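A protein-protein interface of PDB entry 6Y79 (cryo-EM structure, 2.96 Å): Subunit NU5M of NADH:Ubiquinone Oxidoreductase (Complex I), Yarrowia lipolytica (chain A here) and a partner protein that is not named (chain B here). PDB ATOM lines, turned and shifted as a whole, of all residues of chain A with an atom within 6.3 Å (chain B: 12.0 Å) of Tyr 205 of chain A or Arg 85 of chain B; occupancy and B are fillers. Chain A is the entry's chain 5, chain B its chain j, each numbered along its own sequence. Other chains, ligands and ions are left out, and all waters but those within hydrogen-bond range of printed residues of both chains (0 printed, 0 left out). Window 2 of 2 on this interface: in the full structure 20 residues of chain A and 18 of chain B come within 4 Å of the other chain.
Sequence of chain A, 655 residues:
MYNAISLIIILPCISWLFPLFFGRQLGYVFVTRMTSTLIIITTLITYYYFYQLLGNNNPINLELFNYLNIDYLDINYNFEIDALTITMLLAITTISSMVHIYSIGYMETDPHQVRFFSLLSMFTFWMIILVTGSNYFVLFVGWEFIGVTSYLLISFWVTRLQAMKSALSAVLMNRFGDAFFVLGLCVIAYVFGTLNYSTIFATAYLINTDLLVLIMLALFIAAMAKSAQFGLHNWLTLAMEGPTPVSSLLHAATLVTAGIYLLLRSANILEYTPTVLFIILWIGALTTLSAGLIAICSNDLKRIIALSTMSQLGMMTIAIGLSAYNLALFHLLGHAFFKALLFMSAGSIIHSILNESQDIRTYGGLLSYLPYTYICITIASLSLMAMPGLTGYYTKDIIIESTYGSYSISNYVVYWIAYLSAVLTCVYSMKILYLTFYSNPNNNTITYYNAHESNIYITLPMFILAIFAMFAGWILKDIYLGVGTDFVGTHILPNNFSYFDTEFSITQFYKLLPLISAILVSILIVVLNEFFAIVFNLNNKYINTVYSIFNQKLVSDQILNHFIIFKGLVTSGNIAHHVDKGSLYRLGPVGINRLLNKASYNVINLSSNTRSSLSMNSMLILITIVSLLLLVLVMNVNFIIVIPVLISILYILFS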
ATOM      1  N   ILE A 200       7.018 -14.860 -25.234  1.00  0.00           N
ATOM      2  CA  ILE A 200       8.119 -14.138 -25.863  1.00  0.00           C
ATOM      3  C   ILE A 200       7.652 -13.437 -27.131  1.00  0.00           C
ATOM      4  O   ILE A 200       8.021 -12.288 -27.389  1.00  0.00           O
ATOM      5  CB  ILE A 200       9.296 -15.096 -26.123  1.00  0.00           C
ATOM      6  CG1 ILE A 200       9.935 -15.500 -24.804  1.00  0.00           C
ATOM      7  CG2 ILE A 200      10.367 -14.457 -26.958  1.00  0.00           C
ATOM      8  CD1 ILE A 200      10.843 -16.661 -24.936  1.00  0.00           C
ATOM      9  N   PHE A 201       6.786 -14.080 -27.911  1.00  0.00           N
ATOM     10  CA  PHE A 201       6.314 -13.437 -29.132  1.00  0.00           C
ATOM     11  C   PHE A 201       5.193 -12.445 -28.865  1.00  0.00           C
ATOM     12  O   PHE A 201       4.965 -11.556 -29.688  1.00  0.00           O
ATOM     13  CB  PHE A 201       5.844 -14.478 -30.150  1.00  0.00           C
ATOM     14  CG  PHE A 201       6.923 -15.422 -30.599  1.00  0.00           C
ATOM     15  CD1 PHE A 201       8.258 -15.048 -30.568  1.00  0.00           C
ATOM     16  CD2 PHE A 201       6.599 -16.691 -31.043  1.00  0.00           C
ATOM     17  CE1 PHE A 201       9.240 -15.921 -30.961  1.00  0.00           C
ATOM     18  CE2 PHE A 201       7.580 -17.566 -31.439  1.00  0.00           C
ATOM     19  CZ  PHE A 201       8.898 -17.179 -31.395  1.00  0.00           C
ATOM     20  N   ALA A 202       4.492 -12.574 -27.738  1.00  0.00           N
ATOM     21  CA  ALA A 202       3.493 -11.577 -27.379  1.00  0.00           C
ATOM     22  C   ALA A 202       4.134 -10.264 -26.952  1.00  0.00           C
ATOM     23  O   ALA A 202       3.530  -9.202 -27.117  1.00  0.00           O
ATOM     24  CB  ALA A 202       2.597 -12.112 -26.265  1.00  0.00           C
ATOM     25  N   THR A 203       5.350 -10.313 -26.411  1.00  0.00           N
ATOM     26  CA  THR A 203       6.022  -9.139 -25.872  1.00  0.00           C
ATOM     27  C   THR A 203       7.281  -8.774 -26.641  1.00  0.00           C
ATOM     28  O   THR A 203       8.106  -8.021 -26.127  1.00  0.00           O
ATOM     29  CB  THR A 203       6.379  -9.357 -24.404  1.00  0.00           C
ATOM     30  OG1 THR A 203       7.176 -10.540 -24.276  1.00  0.00           O
ATOM     31  CG2 THR A 203       5.142  -9.506 -23.570  1.00  0.00           C
ATOM     32  N   ALA A 204       7.457  -9.293 -27.855  1.00  0.00           N
ATOM     33  CA  ALA A 204       8.718  -9.089 -28.558  1.00  0.00           C
ATOM     34  C   ALA A 204       8.845  -7.690 -29.136  1.00  0.00           C
ATOM     35  O   ALA A 204       9.946  -7.135 -29.155  1.00  0.00           O
ATOM     36  CB  ALA A 204       8.878 -10.111 -29.681  1.00  0.00           C
ATOM     37  N   TYR A 205       7.745  -7.105 -29.604  1.00  0.00           N
ATOM     38  CA  TYR A 205       7.782  -5.803 -30.257  1.00  0.00           C
ATOM     39  C   TYR A 205       8.046  -4.657 -29.293  1.00  0.00           C
ATOM     40  O   TYR A 205       8.363  -3.552 -29.744  1.00  0.00           O
ATOM     41  CB  TYR A 205       6.474  -5.546 -31.020  1.00  0.00           C
ATOM     42  CG  TYR A 205       5.207  -5.441 -30.193  1.00  0.00           C
ATOM     43  CD1 TYR A 205       4.590  -6.574 -29.680  1.00  0.00           C
ATOM     44  CD2 TYR A 205       4.601  -4.214 -29.975  1.00  0.00           C
ATOM     45  CE1 TYR A 205       3.431  -6.483 -28.940  1.00  0.00           C
ATOM     46  CE2 TYR A 205       3.435  -4.114 -29.243  1.00  0.00           C
ATOM     47  CZ  TYR A 205       2.859  -5.253 -28.724  1.00  0.00           C
ATOM     48  OH  TYR A 205       1.700  -5.167 -27.990  1.00  0.00           O
ATOM     49  N   LEU A 206       7.934  -4.890 -27.992  1.00  0.00           N
ATOM     50  CA  LEU A 206       8.173  -3.848 -27.013  1.00  0.00           C
ATOM     51  C   LEU A 206       9.624  -3.751 -26.581  1.00  0.00           C
ATOM     52  O   LEU A 206      10.069  -2.655 -26.251  1.00  0.00           O
ATOM     53  CB  LEU A 206       7.285  -4.081 -25.795  1.00  0.00           C
ATOM     54  CG  LEU A 206       5.824  -4.046 -26.222  1.00  0.00           C
ATOM     55  CD1 LEU A 206       4.892  -4.458 -25.099  1.00  0.00           C
ATOM     56  CD2 LEU A 206       5.501  -2.656 -26.725  1.00  0.00           C
ATOM     57  N   ILE A 207      10.370  -4.857 -26.623  1.00  0.00           N
ATOM     58  CA  ILE A 207      11.720  -4.933 -26.072  1.00  0.00           C
ATOM     59  C   ILE A 207      12.687  -4.084 -26.898  1.00  0.00           C
ATOM     60  O   ILE A 207      12.492  -3.879 -28.102  1.00  0.00           O
ATOM     61  CB  ILE A 207      12.121  -6.420 -26.020  1.00  0.00           C
ATOM     62  CG1 ILE A 207      11.117  -7.177 -25.161  1.00  0.00           C
ATOM     63  CG2 ILE A 207      13.509  -6.667 -25.448  1.00  0.00           C
ATOM     64  CD1 ILE A 207      11.076  -6.718 -23.735  1.00  0.00           C
ATOM     65  N   ASN A 208      13.700  -3.530 -26.218  1.00  0.00           N
ATOM     66  CA  ASN A 208      14.737  -2.718 -26.840  1.00  0.00           C
ATOM     67  C   ASN A 208      15.471  -3.480 -27.934  1.00  0.00           C
ATOM     68  O   ASN A 208      15.621  -4.701 -27.875  1.00  0.00           O
ATOM     69  CB  ASN A 208      15.740  -2.253 -25.785  1.00  0.00           C
ATOM     70  CG  ASN A 208      16.618  -1.119 -26.276  1.00  0.00           C
ATOM     71  OD1 ASN A 208      16.418  -0.586 -27.366  1.00  0.00           O
ATOM     72  ND2 ASN A 208      17.599  -0.750 -25.479  1.00  0.00           N
ATOM     73  N   THR A 209      15.945  -2.740 -28.935  1.00  0.00           N
ATOM     74  CA  THR A 209      16.483  -3.388 -30.122  1.00  0.00           C
ATOM     75  C   THR A 209      17.933  -3.825 -29.944  1.00  0.00           C
ATOM     76  O   THR A 209      18.372  -4.751 -30.630  1.00  0.00           O
ATOM     77  CB  THR A 209      16.318  -2.474 -31.338  1.00  0.00           C
ATOM     78  OG1 THR A 209      16.734  -3.170 -32.518  1.00  0.00           O
ATOM     79  CG2 THR A 209      17.117  -1.189 -31.192  1.00  0.00           C
ATOM     80  N   LEU A 212      17.679  -7.233 -28.445  1.00  0.00           N
ATOM     81  CA  LEU A 212      17.268  -8.229 -29.423  1.00  0.00           C
ATOM     82  C   LEU A 212      18.369  -8.509 -30.435  1.00  0.00           C
ATOM     83  O   LEU A 212      18.473  -9.630 -30.938  1.00  0.00           O
ATOM     84  CB  LEU A 212      15.988  -7.773 -30.113  1.00  0.00           C
ATOM     85  CG  LEU A 212      14.738  -7.930 -29.246  1.00  0.00           C
ATOM     86  CD1 LEU A 212      13.512  -7.719 -30.081  1.00  0.00           C
ATOM     87  CD2 LEU A 212      14.669  -9.284 -28.554  1.00  0.00           C
ATOM     88  N   ASN A 268       9.457 -14.432 -35.526  1.00  0.00           N
ATOM     89  CA  ASN A 268       8.601 -13.401 -34.932  1.00  0.00           C
ATOM     90  C   ASN A 268       9.390 -12.424 -34.070  1.00  0.00           C
ATOM     91  O   ASN A 268       8.981 -11.274 -33.907  1.00  0.00           O
ATOM     92  CB  ASN A 268       7.494 -14.039 -34.096  1.00  0.00           C
ATOM     93  CG  ASN A 268       6.438 -14.696 -34.936  1.00  0.00           C
ATOM     94  OD1 ASN A 268       6.006 -14.150 -35.944  1.00  0.00           O
ATOM     95  ND2 ASN A 268       6.008 -15.879 -34.524  1.00  0.00           N
ATOM     96  N   TYR A 272      11.869  -7.536 -35.664  1.00  0.00           N
ATOM     97  CA  TYR A 272      12.100  -6.260 -35.009  1.00  0.00           C
ATOM     98  C   TYR A 272      13.571  -5.907 -34.943  1.00  0.00           C
ATOM     99  O   TYR A 272      13.944  -4.952 -34.256  1.00  0.00           O
ATOM    100  CB  TYR A 272      11.462  -6.309 -33.627  1.00  0.00           C
ATOM    101  CG  TYR A 272       9.984  -6.473 -33.799  1.00  0.00           C
ATOM    102  CD1 TYR A 272       9.205  -5.390 -34.158  1.00  0.00           C
ATOM    103  CD2 TYR A 272       9.373  -7.715 -33.678  1.00  0.00           C
ATOM    104  CE1 TYR A 272       7.866  -5.522 -34.344  1.00  0.00           C
ATOM    105  CE2 TYR A 272       8.025  -7.858 -33.878  1.00  0.00           C
ATOM    106  CZ  TYR A 272       7.279  -6.753 -34.212  1.00  0.00           C
ATOM    107  OH  TYR A 272       5.928  -6.860 -34.411  1.00  0.00           O
ATOM    108  N   GLU B  79      21.502  -2.961 -17.007  1.00  0.00           N
ATOM    109  CA  GLU B  79      20.265  -3.668 -16.723  1.00  0.00           C
ATOM    110  C   GLU B  79      19.558  -3.919 -18.051  1.00  0.00           C
ATOM    111  O   GLU B  79      19.484  -3.029 -18.902  1.00  0.00           O
ATOM    112  CB  GLU B  79      19.378  -2.886 -15.737  1.00  0.00           C
ATOM    113  CG  GLU B  79      19.008  -1.469 -16.166  1.00  0.00           C
ATOM    114  CD  GLU B  79      18.011  -0.777 -15.249  1.00  0.00           C
ATOM    115  OE1 GLU B  79      17.690  -1.309 -14.162  1.00  0.00           O
ATOM    116  OE2 GLU B  79      17.481   0.285 -15.662  1.00  0.00           O
ATOM    117  N   PHE B  80      19.128  -5.162 -18.275  1.00  0.00           N
ATOM    118  CA  PHE B  80      18.376  -5.520 -19.474  1.00  0.00           C
ATOM    119  C   PHE B  80      17.002  -6.079 -19.131  1.00  0.00           C
ATOM    120  O   PHE B  80      16.390  -6.731 -19.977  1.00  0.00           O
ATOM    121  CB  PHE B  80      19.094  -6.565 -20.339  1.00  0.00           C
ATOM    122  CG  PHE B  80      20.466  -6.190 -20.813  1.00  0.00           C
ATOM    123  CD1 PHE B  80      20.825  -4.879 -21.052  1.00  0.00           C
ATOM    124  CD2 PHE B  80      21.387  -7.185 -21.074  1.00  0.00           C
ATOM    125  CE1 PHE B  80      22.077  -4.568 -21.513  1.00  0.00           C
ATOM    126  CE2 PHE B  80      22.648  -6.879 -21.535  1.00  0.00           C
ATOM    127  CZ  PHE B  80      22.992  -5.570 -21.753  1.00  0.00           C
ATOM    128  N   ALA B  81      16.508  -5.850 -17.913  1.00  0.00           N
ATOM    129  CA  ALA B  81      15.396  -6.649 -17.399  1.00  0.00           C
ATOM    130  C   ALA B  81      14.083  -6.306 -18.091  1.00  0.00           C
ATOM    131  O   ALA B  81      13.517  -7.133 -18.807  1.00  0.00           O
ATOM    132  CB  ALA B  81      15.276  -6.458 -15.890  1.00  0.00           C
ATOM    133  N   GLY B  82      13.589  -5.091 -17.912  1.00  0.00           N
ATOM    134  CA  GLY B  82      12.484  -4.657 -18.742  1.00  0.00           C
ATOM    135  C   GLY B  82      12.826  -3.372 -19.459  1.00  0.00           C
ATOM    136  O   GLY B  82      12.902  -2.312 -18.830  1.00  0.00           O
ATOM    137  N   LYS B  83      13.017  -3.444 -20.772  1.00  0.00           N
ATOM    138  CA  LYS B  83      13.488  -2.308 -21.542  1.00  0.00           C
ATOM    139  C   LYS B  83      12.655  -2.160 -22.800  1.00  0.00           C
ATOM    140  O   LYS B  83      11.983  -3.095 -23.235  1.00  0.00           O
ATOM    141  CB  LYS B  83      14.966  -2.447 -21.901  1.00  0.00           C
ATOM    142  CG  LYS B  83      15.880  -2.290 -20.706  1.00  0.00           C
ATOM    143  CD  LYS B  83      15.636  -0.948 -20.033  1.00  0.00           C
ATOM    144  CE  LYS B  83      16.318  -0.870 -18.681  1.00  0.00           C
ATOM    145  NZ  LYS B  83      15.722  -1.824 -17.720  1.00  0.00           N
ATOM    146  N   ARG B  84      12.695  -0.963 -23.380  1.00  0.00           N
ATOM    147  CA  ARG B  84      11.903  -0.664 -24.558  1.00  0.00           C
ATOM    148  C   ARG B  84      12.732   0.096 -25.580  1.00  0.00           C
ATOM    149  O   ARG B  84      13.893   0.427 -25.343  1.00  0.00           O
ATOM    150  CB  ARG B  84      10.653   0.131 -24.212  1.00  0.00           C
ATOM    151  CG  ARG B  84       9.549  -0.677 -23.567  1.00  0.00           C
ATOM    152  CD  ARG B  84       9.620  -0.554 -22.068  1.00  0.00           C
ATOM    153  NE  ARG B  84       8.381  -0.961 -21.427  1.00  0.00           N
ATOM    154  CZ  ARG B  84       8.105  -2.211 -21.099  1.00  0.00           C
ATOM    155  NH1 ARG B  84       8.987  -3.164 -21.370  1.00  0.00           N
ATOM    156  NH2 ARG B  84       6.955  -2.504 -20.512  1.00  0.00           N
ATOM    157  N   ARG B  85      12.118   0.362 -26.732  1.00  0.00           N
ATOM    158  CA  ARG B  85      12.825   1.054 -27.800  1.00  0.00           C
ATOM    159  C   ARG B  85      12.969   2.535 -27.480  1.00  0.00           C
ATOM    160  O   ARG B  85      11.981   3.248 -27.290  1.00  0.00           O
ATOM    161  CB  ARG B  85      12.102   0.903 -29.133  1.00  0.00           C
ATOM    162  CG  ARG B  85      11.448  -0.415 -29.393  1.00  0.00           C
ATOM    163  CD  ARG B  85      10.795  -0.351 -30.749  1.00  0.00           C
ATOM    164  NE  ARG B  85       9.828  -1.413 -30.967  1.00  0.00           N
ATOM    165  CZ  ARG B  85       9.126  -1.543 -32.083  1.00  0.00           C
ATOM    166  NH1 ARG B  85       9.289  -0.672 -33.067  1.00  0.00           N
ATOM    167  NH2 ARG B  85       8.261  -2.536 -32.217  1.00  0.00           N
ATOM    168  N   GLY B  86      14.210   3.002 -27.472  1.00  0.00           N
ATOM    169  CA  GLY B  86      14.512   4.352 -27.070  1.00  0.00           C
ATOM    170  C   GLY B  86      14.888   4.500 -25.618  1.00  0.00           C
ATOM    171  O   GLY B  86      15.022   5.633 -25.140  1.00  0.00           O
ATOM    172  N   GLU B  87      15.060   3.398 -24.902  1.00  0.00           N
ATOM    173  CA  GLU B  87      15.392   3.419 -23.488  1.00  0.00           C
ATOM    174  C   GLU B  87      16.827   2.968 -23.300  1.00  0.00           C
ATOM    175  O   GLU B  87      17.290   2.038 -23.970  1.00  0.00           O
ATOM    176  CB  GLU B  87      14.444   2.526 -22.680  1.00  0.00           C
ATOM    177  CG  GLU B  87      13.152   3.202 -22.209  1.00  0.00           C
ATOM    178  CD  GLU B  87      12.084   3.294 -23.292  1.00  0.00           C
ATOM    179  OE1 GLU B  87      12.384   2.991 -24.458  1.00  0.00           O
ATOM    180  OE2 GLU B  87      10.930   3.644 -22.984  1.00  0.00           O
ATOM    181  N   SER B  88      17.528   3.664 -22.415  1.00  0.00           N
ATOM    182  CA  SER B  88      18.865   3.269 -22.008  1.00  0.00           C
ATOM    183  C   SER B  88      18.842   1.902 -21.352  1.00  0.00           C
ATOM    184  O   SER B  88      17.877   1.536 -20.673  1.00  0.00           O
ATOM    185  CB  SER B  88      19.424   4.277 -21.026  1.00  0.00           C
ATOM    186  OG  SER B  88      18.669   4.221 -19.827  1.00  0.00           O
ATOM    187  N   VAL B  89      19.907   1.129 -21.587  1.00  0.00           N
ATOM    188  CA  VAL B  89      20.112  -0.104 -20.841  1.00  0.00           C
ATOM    189  C   VAL B  89      21.303  -0.023 -19.914  1.00  0.00           C
ATOM    190  O   VAL B  89      21.492  -0.922 -19.085  1.00  0.00           O
ATOM    191  CB  VAL B  89      20.244  -1.298 -21.799  1.00  0.00           C
ATOM    192  CG1 VAL B  89      18.977  -1.444 -22.546  1.00  0.00           C
ATOM    193  CG2 VAL B  89      21.409  -1.104 -22.755  1.00  0.00           C
ATOM    194  N   THR B  90      22.106   1.024 -20.017  1.00  0.00           N
ATOM    195  CA  THR B  90      23.129   1.299 -19.031  1.00  0.00           C
ATOM    196  C   THR B  90      22.617   2.337 -18.042  1.00  0.00           C
ATOM    197  O   THR B  90      21.526   2.889 -18.184  1.00  0.00           O
ATOM    198  CB  THR B  90      24.427   1.763 -19.687  1.00  0.00           C
ATOM    199  OG1 THR B  90      24.191   2.977 -20.405  1.00  0.00           O
ATOM    200  CG2 THR B  90      24.908   0.721 -20.644  1.00  0.00           C
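Of the 12 printed residues of chain B, 5 touch a printed residue of chain A. Along chain A the printed residues that touch a printed residue of chain B span positions 205 to 272.
The side-chain carboxylate (OE2) of Glu 79 of chain B is in salt-bridge range of the side-chain amino group (NZ) of Lys 83 of chain B (3.4 Å). The backbone NH of Arg 85 of chain B sits close to the side-chain carboxylate of Glu 87 of chain B. The backbone NH (N) of Glu 79 of chain B sits at hydrogen-bond distance from the backbone carbonyl oxygen (O) of Val 89 of chain B (2.9 Å).
No residue of chain B comes within 4 Å of Thr 203 of chain A. No residue of chain B comes within 4 Å of Ala 204 of chain A. Of chain B, only Arg 85 comes within 4 Å of Tyr 205 of chain A. Leu 206 of chain A touches just these residues of chain B: Lys 83, Arg 84 and Arg 85. Ile 207 of chain A touches just these residues of chain B: Lys 83 (3.4 Å) and Arg 85 (3.8 Å). Of chain B, only Lys 83 (3.5 Å), Arg 84 (3.3 Å), Arg 85 (3.97 Å), Glu 87 (3.2 Å) and Val 89 (3.3 Å) come within 4 Å of Asn 208 of chain A. Asn 268 of chain A touches none of the printed residues of chain B. Tyr 272 of chain A touches just one residue of chain B: Arg 85 (3.6 Å). Phe 80 of chain B touches none of the printed residues of chain A. Printed residues of chain A within 4 Å of Lys 83 of chain B: Leu 206 (3.6 Å), Ile 207 (3.4 Å) and Asn 208 (3.5 Å). Printed residues of chain A within 4 Å of Arg 84 of chain B: Leu 206 and Asn 208. Arg 85 of chain B touches just these residues of chain A: Tyr 205, Leu 206, Ile 207, Asn 208 and Tyr 272. Printed residues of chain A within 4 Å of Glu 87 of chain B: Asn 208 (3.2 Å). Of the printed residues of chain A, Val 89 of chain B touches Asn 208. The nearest residue of chain B that does not touch Tyr 205 of chain A is Arg 84 of chain B (6.9 Å). The nearest residue of chain A that does not touch Arg 85 of chain B is Thr 209 of chain A (5.0 Å).
NH2 of Arg 85 of chain B lies within hydrogen-bond range of O of Tyr 205 of chain A (2.7 Å). O of Arg 84 of chain B sits close to OD1 of Asn 208 of chain A (3.4 Å). The side-chain amide nitrogen (ND2) of Asn 208 of chain A is in hydrogen-bond range of the backbone carbonyl oxygen (O) of Glu 87 of chain B. O of Lys 83 of chain B sits at hydrogen-bond distance from N of Asn 208 of chain A (3.5 Å).
Among the printed residues, pairs that only touch across the chains: Leu 206 of chain A with Lys 83 of chain B, Leu 206 of chain A with Arg 84 of chain B, Leu 206 of chain A with Arg 85 of chain B, Ile 207 of chain A with Lys 83 of chain B, Ile 207 of chain A with Arg 85 of chain B, Asn 208 of chain A with Arg 85 of chain B, Asn 208 of chain A with Val 89 of chain B and Tyr 272 of chain A with Arg 85 of chain B.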
